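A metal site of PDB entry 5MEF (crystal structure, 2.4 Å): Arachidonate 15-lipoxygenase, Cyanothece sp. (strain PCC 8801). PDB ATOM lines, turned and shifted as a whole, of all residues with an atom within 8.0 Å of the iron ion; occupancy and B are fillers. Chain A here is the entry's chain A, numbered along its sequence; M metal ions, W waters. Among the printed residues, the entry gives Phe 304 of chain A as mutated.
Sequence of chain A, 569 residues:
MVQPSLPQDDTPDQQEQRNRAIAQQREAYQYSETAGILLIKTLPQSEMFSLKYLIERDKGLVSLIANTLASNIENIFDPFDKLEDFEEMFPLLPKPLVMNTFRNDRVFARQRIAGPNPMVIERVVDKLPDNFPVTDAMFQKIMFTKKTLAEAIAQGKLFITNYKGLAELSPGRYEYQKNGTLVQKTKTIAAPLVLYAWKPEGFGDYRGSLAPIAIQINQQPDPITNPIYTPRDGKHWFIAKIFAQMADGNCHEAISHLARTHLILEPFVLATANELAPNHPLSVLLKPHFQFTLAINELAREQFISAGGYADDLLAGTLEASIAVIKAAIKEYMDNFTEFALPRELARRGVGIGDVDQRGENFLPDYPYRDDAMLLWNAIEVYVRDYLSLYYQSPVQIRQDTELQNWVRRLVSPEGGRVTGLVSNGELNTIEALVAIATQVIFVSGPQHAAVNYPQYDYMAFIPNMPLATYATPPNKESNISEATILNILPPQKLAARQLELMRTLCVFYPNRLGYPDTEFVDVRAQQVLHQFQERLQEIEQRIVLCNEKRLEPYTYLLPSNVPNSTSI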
ATOM      1  N   HIS A 252      17.291   5.638 -11.944  1.00  0.00           N
ATOM      2  CA  HIS A 252      18.385   5.788 -12.903  1.00  0.00           C
ATOM      3  C   HIS A 252      19.419   6.804 -12.416  1.00  0.00           C
ATOM      4  O   HIS A 252      20.617   6.514 -12.359  1.00  0.00           O
ATOM      5  CB  HIS A 252      17.836   6.211 -14.271  1.00  0.00           C
ATOM      6  CG  HIS A 252      18.884   6.754 -15.203  1.00  0.00           C
ATOM      7  ND1 HIS A 252      19.246   8.086 -15.196  1.00  0.00           N
ATOM      8  CD2 HIS A 252      19.647   6.157 -16.146  1.00  0.00           C
ATOM      9  CE1 HIS A 252      20.187   8.280 -16.103  1.00  0.00           C
ATOM     10  NE2 HIS A 252      20.447   7.126 -16.691  1.00  0.00           N
ATOM     11  N   GLU A 253      18.956   8.004 -12.050  1.00  0.00           N
ATOM     12  CA  GLU A 253      19.900   9.063 -11.690  1.00  0.00           C
ATOM     13  C   GLU A 253      20.576   8.798 -10.356  1.00  0.00           C
ATOM     14  O   GLU A 253      21.785   8.989 -10.223  1.00  0.00           O
ATOM     15  CB  GLU A 253      19.194  10.419 -11.679  1.00  0.00           C
ATOM     16  CG  GLU A 253      18.700  10.878 -13.062  1.00  0.00           C
ATOM     17  CD  GLU A 253      19.846  11.149 -14.056  1.00  0.00           C
ATOM     18  OE1 GLU A 253      21.026  11.053 -13.678  1.00  0.00           O
ATOM     19  OE2 GLU A 253      19.542  11.455 -15.223  1.00  0.00           O
ATOM     20  N   HIS A 257      23.188   5.715 -12.265  1.00  0.00           N
ATOM     21  CA  HIS A 257      24.118   6.671 -12.877  1.00  0.00           C
ATOM     22  C   HIS A 257      25.102   7.222 -11.843  1.00  0.00           C
ATOM     23  O   HIS A 257      26.279   6.848 -11.846  1.00  0.00           O
ATOM     24  CB  HIS A 257      23.330   7.802 -13.548  1.00  0.00           C
ATOM     25  CG  HIS A 257      24.192   8.780 -14.282  1.00  0.00           C
ATOM     26  ND1 HIS A 257      23.828  10.100 -14.468  1.00  0.00           N
ATOM     27  CD2 HIS A 257      25.389   8.639 -14.887  1.00  0.00           C
ATOM     28  CE1 HIS A 257      24.773  10.722 -15.146  1.00  0.00           C
ATOM     29  NE2 HIS A 257      25.733   9.859 -15.418  1.00  0.00           N
ATOM     30  N   LEU A 258      24.629   8.097 -10.948  1.00  0.00           N
ATOM     31  CA  LEU A 258      25.524   8.730  -9.989  1.00  0.00           C
ATOM     32  C   LEU A 258      26.209   7.719  -9.095  1.00  0.00           C
ATOM     33  O   LEU A 258      27.439   7.709  -8.961  1.00  0.00           O
ATOM     34  CB  LEU A 258      24.764   9.772  -9.159  1.00  0.00           C
ATOM     35  CG  LEU A 258      24.605  11.139  -9.815  1.00  0.00           C
ATOM     36  CD1 LEU A 258      23.753  12.051  -8.962  1.00  0.00           C
ATOM     37  CD2 LEU A 258      25.979  11.746 -10.063  1.00  0.00           C
ATOM     38  N   THR A 261      28.120   4.380 -11.298  1.00  0.00           N
ATOM     39  CA  THR A 261      29.199   4.624 -12.248  1.00  0.00           C
ATOM     40  C   THR A 261      30.143   5.673 -11.671  1.00  0.00           C
ATOM     41  O   THR A 261      31.270   5.350 -11.313  1.00  0.00           O
ATOM     42  CB  THR A 261      28.661   5.051 -13.623  1.00  0.00           C
ATOM     43  OG1 THR A 261      27.854   6.217 -13.489  1.00  0.00           O
ATOM     44  CG2 THR A 261      27.854   3.918 -14.247  1.00  0.00           C
ATOM     45  N   HIS A 262      29.674   6.920 -11.565  1.00  0.00           N
ATOM     46  CA  HIS A 262      30.524   8.022 -11.117  1.00  0.00           C
ATOM     47  C   HIS A 262      31.146   7.756  -9.756  1.00  0.00           C
ATOM     48  O   HIS A 262      32.371   7.768  -9.602  1.00  0.00           O
ATOM     49  CB  HIS A 262      29.731   9.329 -11.079  1.00  0.00           C
ATOM     50  CG  HIS A 262      29.362   9.862 -12.425  1.00  0.00           C
ATOM     51  ND1 HIS A 262      30.045  10.890 -13.032  1.00  0.00           N
ATOM     52  CD2 HIS A 262      28.381   9.509 -13.298  1.00  0.00           C
ATOM     53  CE1 HIS A 262      29.505  11.160 -14.204  1.00  0.00           C
ATOM     54  NE2 HIS A 262      28.496  10.335 -14.389  1.00  0.00           N
ATOM     55  N   ILE A 296      34.930  15.255 -13.204  1.00  0.00           N
ATOM     56  CA  ILE A 296      33.483  15.209 -13.410  1.00  0.00           C
ATOM     57  C   ILE A 296      32.758  14.894 -12.113  1.00  0.00           C
ATOM     58  O   ILE A 296      31.609  15.312 -11.925  1.00  0.00           O
ATOM     59  CB  ILE A 296      33.136  14.198 -14.516  1.00  0.00           C
ATOM     60  CG1 ILE A 296      31.678  14.377 -14.959  1.00  0.00           C
ATOM     61  CG2 ILE A 296      33.361  12.764 -14.050  1.00  0.00           C
ATOM     62  CD1 ILE A 296      31.389  15.690 -15.632  1.00  0.00           C
ATOM     63  N   ASN A 297      33.394  14.186 -11.184  1.00  0.00           N
ATOM     64  CA  ASN A 297      32.772  13.942  -9.889  1.00  0.00           C
ATOM     65  C   ASN A 297      32.776  15.197  -9.028  1.00  0.00           C
ATOM     66  O   ASN A 297      31.861  15.395  -8.219  1.00  0.00           O
ATOM     67  CB  ASN A 297      33.467  12.796  -9.151  1.00  0.00           C
ATOM     68  CG  ASN A 297      33.007  11.431  -9.642  1.00  0.00           C
ATOM     69  OD1 ASN A 297      31.943  11.313 -10.242  1.00  0.00           O
ATOM     70  ND2 ASN A 297      33.795  10.403  -9.353  1.00  0.00           N
ATOM     71  N   ALA A 300      29.869  17.121 -10.301  1.00  0.00           N
ATOM     72  CA  ALA A 300      28.656  16.537  -9.728  1.00  0.00           C
ATOM     73  C   ALA A 300      28.480  16.969  -8.282  1.00  0.00           C
ATOM     74  O   ALA A 300      27.343  17.188  -7.825  1.00  0.00           O
ATOM     75  CB  ALA A 300      28.711  15.014  -9.841  1.00  0.00           C
ATOM     76  N   PHE A 304      25.410  18.866  -9.186  1.00  0.00           N
ATOM     77  CA  PHE A 304      24.420  17.796  -9.247  1.00  0.00           C
ATOM     78  C   PHE A 304      23.795  17.479  -7.892  1.00  0.00           C
ATOM     79  O   PHE A 304      22.571  17.465  -7.765  1.00  0.00           O
ATOM     80  CB  PHE A 304      25.053  16.538  -9.858  1.00  0.00           C
ATOM     81  CG  PHE A 304      24.097  15.714 -10.672  1.00  0.00           C
ATOM     82  CD1 PHE A 304      24.545  15.055 -11.819  1.00  0.00           C
ATOM     83  CD2 PHE A 304      22.780  15.560 -10.294  1.00  0.00           C
ATOM     84  CE1 PHE A 304      23.670  14.287 -12.568  1.00  0.00           C
ATOM     85  CE2 PHE A 304      21.904  14.792 -11.043  1.00  0.00           C
ATOM     86  CZ  PHE A 304      22.349  14.156 -12.180  1.00  0.00           C
ATOM     87  N   HIS A 449      29.020   3.166 -17.948  1.00  0.00           N
ATOM     88  CA  HIS A 449      28.677   4.588 -17.907  1.00  0.00           C
ATOM     89  C   HIS A 449      28.125   5.045 -19.244  1.00  0.00           C
ATOM     90  O   HIS A 449      27.201   5.858 -19.285  1.00  0.00           O
ATOM     91  CB  HIS A 449      29.891   5.431 -17.540  1.00  0.00           C
ATOM     92  CG  HIS A 449      29.609   6.903 -17.512  1.00  0.00           C
ATOM     93  ND1 HIS A 449      30.013   7.754 -18.522  1.00  0.00           N
ATOM     94  CD2 HIS A 449      28.896   7.671 -16.644  1.00  0.00           C
ATOM     95  CE1 HIS A 449      29.609   8.983 -18.253  1.00  0.00           C
ATOM     96  NE2 HIS A 449      28.925   8.958 -17.125  1.00  0.00           N
ATOM     97  N   ALA A 450      28.669   4.538 -20.350  1.00  0.00           N
ATOM     98  CA  ALA A 450      28.114   4.865 -21.649  1.00  0.00           C
ATOM     99  C   ALA A 450      26.660   4.427 -21.742  1.00  0.00           C
ATOM    100  O   ALA A 450      25.809   5.153 -22.284  1.00  0.00           O
ATOM    101  CB  ALA A 450      28.931   4.209 -22.756  1.00  0.00           C
ATOM    102  N   VAL A 452      24.317   3.975 -19.424  1.00  0.00           N
ATOM    103  CA  VAL A 452      23.375   4.759 -18.630  1.00  0.00           C
ATOM    104  C   VAL A 452      23.407   6.269 -18.919  1.00  0.00           C
ATOM    105  O   VAL A 452      22.367   6.923 -18.881  1.00  0.00           O
ATOM    106  CB  VAL A 452      23.598   4.486 -17.121  1.00  0.00           C
ATOM    107  CG1 VAL A 452      23.389   3.007 -16.797  1.00  0.00           C
ATOM    108  CG2 VAL A 452      24.967   4.943 -16.688  1.00  0.00           C
ATOM    109  N   ASN A 453      24.582   6.854 -19.201  1.00  0.00           N
ATOM    110  CA  ASN A 453      24.667   8.288 -19.498  1.00  0.00           C
ATOM    111  C   ASN A 453      24.115   8.733 -20.856  1.00  0.00           C
ATOM    112  O   ASN A 453      23.347   9.693 -20.933  1.00  0.00           O
ATOM    113  CB  ASN A 453      26.132   8.703 -19.361  1.00  0.00           C
ATOM    114  CG  ASN A 453      26.343  10.191 -19.507  1.00  0.00           C
ATOM    115  OD1 ASN A 453      26.384  10.932 -18.513  1.00  0.00           O
ATOM    116  ND2 ASN A 453      26.491  10.649 -20.743  1.00  0.00           N
ATOM    117  N   TYR A 454      24.492   8.069 -21.950  1.00  0.00           N
ATOM    118  CA  TYR A 454      24.064   8.508 -23.284  1.00  0.00           C
ATOM    119  C   TYR A 454      22.585   8.426 -23.676  1.00  0.00           C
ATOM    120  O   TYR A 454      22.103   9.334 -24.371  1.00  0.00           O
ATOM    121  CB  TYR A 454      24.976   7.945 -24.362  1.00  0.00           C
ATOM    122  CG  TYR A 454      26.318   8.656 -24.242  1.00  0.00           C
ATOM    123  CD1 TYR A 454      26.455   9.947 -24.745  1.00  0.00           C
ATOM    124  CD2 TYR A 454      27.411   8.079 -23.598  1.00  0.00           C
ATOM    125  CE1 TYR A 454      27.656  10.644 -24.634  1.00  0.00           C
ATOM    126  CE2 TYR A 454      28.620   8.781 -23.485  1.00  0.00           C
ATOM    127  CZ  TYR A 454      28.729  10.068 -24.006  1.00  0.00           C
ATOM    128  OH  TYR A 454      29.908  10.765 -23.901  1.00  0.00           O
ATOM    129  N   GLN A 456      20.231   9.218 -21.946  1.00  0.00           N
ATOM    130  CA  GLN A 456      19.527  10.216 -21.153  1.00  0.00           C
ATOM    131  C   GLN A 456      18.856  11.280 -22.031  1.00  0.00           C
ATOM    132  O   GLN A 456      17.719  11.679 -21.768  1.00  0.00           O
ATOM    133  CB  GLN A 456      20.500  10.898 -20.192  1.00  0.00           C
ATOM    134  CG  GLN A 456      20.796  10.121 -18.923  1.00  0.00           C
ATOM    135  CD  GLN A 456      21.802  10.832 -18.046  1.00  0.00           C
ATOM    136  OE1 GLN A 456      22.946  11.067 -18.449  1.00  0.00           O
ATOM    137  NE2 GLN A 456      21.385  11.189 -16.835  1.00  0.00           N
ATOM    138  N   LEU A 506      24.888  16.402 -20.413  1.00  0.00           N
ATOM    139  CA  LEU A 506      25.403  15.054 -20.218  1.00  0.00           C
ATOM    140  C   LEU A 506      25.708  14.310 -21.521  1.00  0.00           C
ATOM    141  O   LEU A 506      26.683  13.544 -21.579  1.00  0.00           O
ATOM    142  CB  LEU A 506      24.446  14.248 -19.340  1.00  0.00           C
ATOM    143  CG  LEU A 506      24.238  14.846 -17.951  1.00  0.00           C
ATOM    144  CD1 LEU A 506      23.390  13.937 -17.066  1.00  0.00           C
ATOM    145  CD2 LEU A 506      25.559  15.195 -17.285  1.00  0.00           C
ATOM    146  N   CYS A 507      24.905  14.479 -22.570  1.00  0.00           N
ATOM    147  CA  CYS A 507      25.154  13.738 -23.806  1.00  0.00           C
ATOM    148  C   CYS A 507      25.645  14.579 -24.979  1.00  0.00           C
ATOM    149  O   CYS A 507      25.501  14.150 -26.129  1.00  0.00           O
ATOM    150  CB  CYS A 507      23.895  12.990 -24.225  1.00  0.00           C
ATOM    151  SG  CYS A 507      22.889  12.357 -22.879  1.00  0.00           S
ATOM    152  N   THR A 567      34.742   7.379 -17.464  1.00  0.00           N
ATOM    153  CA  THR A 567      33.574   8.131 -16.994  1.00  0.00           C
ATOM    154  C   THR A 567      33.995   9.591 -16.895  1.00  0.00           C
ATOM    155  O   THR A 567      34.689   9.992 -15.956  1.00  0.00           O
ATOM    156  CB  THR A 567      33.082   7.586 -15.658  1.00  0.00           C
ATOM    157  OG1 THR A 567      32.561   6.259 -15.844  1.00  0.00           O
ATOM    158  CG2 THR A 567      31.989   8.474 -15.090  1.00  0.00           C
ATOM    159  N   SER A 568      33.582  10.388 -17.874  1.00  0.00           N
ATOM    160  CA  SER A 568      34.156  11.715 -18.027  1.00  0.00           C
ATOM    161  C   SER A 568      33.137  12.794 -18.368  1.00  0.00           C
ATOM    162  O   SER A 568      33.534  13.919 -18.678  1.00  0.00           O
ATOM    163  CB  SER A 568      35.255  11.689 -19.092  1.00  0.00           C
ATOM    164  OG  SER A 568      34.808  10.960 -20.230  1.00  0.00           O
ATOM    165  N   ILE A 569      31.836  12.487 -18.342  1.00  0.00           N
ATOM    166  CA  ILE A 569      30.839  13.503 -18.648  1.00  0.00           C
ATOM    167  C   ILE A 569      29.584  13.231 -17.799  1.00  0.00           C
ATOM    168  O   ILE A 569      29.391  12.120 -17.338  1.00  0.00           O
ATOM    169  CB  ILE A 569      30.506  13.535 -20.152  1.00  0.00           C
ATOM    170  CG1 ILE A 569      29.667  14.766 -20.503  1.00  0.00           C
ATOM    171  CG2 ILE A 569      29.787  12.253 -20.579  1.00  0.00           C
ATOM    172  CD1 ILE A 569      29.466  14.962 -21.997  1.00  0.00           C
ATOM    173  OXT ILE A 569      28.752  14.117 -17.564  1.00  0.00           O
HETATM  174 FE    FE M   1      27.655  10.748 -16.493  1.00  0.00          FE
HETATM  175  O   HOH W   1      26.854  12.655 -15.924  1.00  0.00           O
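ND2 of Asn 297 lies within hydrogen-bond range of O of His 262 (3.0 Å).
A ring nitrogen (ND1) of His 257 sits at hydrogen-bond distance from the side-chain carboxylate (OE1) of Glu 253 (3.1 Å).
N of His 257 sits at hydrogen-bond distance from O of His 252.
The side-chain amide nitrogen (ND2) of Asn 453 lies within hydrogen-bond range of the backbone carbonyl oxygen (O) of Leu 506, 3.0 Å away.
The side-chain amide oxygen (OE1) of Gln 456 lies close to the backbone carbonyl oxygen (O) of Asn 453 (2.9 Å).
The backbone carbonyl oxygen (O) of Asn 453 is in hydrogen-bond range of the side-chain sulfur (SG) of Cys 507 (3.3 Å).
The nearest printed residue that does not touch the iron ion is Leu 506 (5.0 Å).
Water W1 binds the iron ion, at 2.1 Å.
NE2 of His 449 binds the iron ion.
NE2 of His 262 is bound to the iron ion, 2.3 Å away.
O of Ile 569 is bound to the iron ion (2.4 Å).
The iron ion is bound by NE2 of His 257, 2.4 Å away.
The side-chain amide oxygen (OD1) of Asn 453 is bound to the iron ion (2.4 Å).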
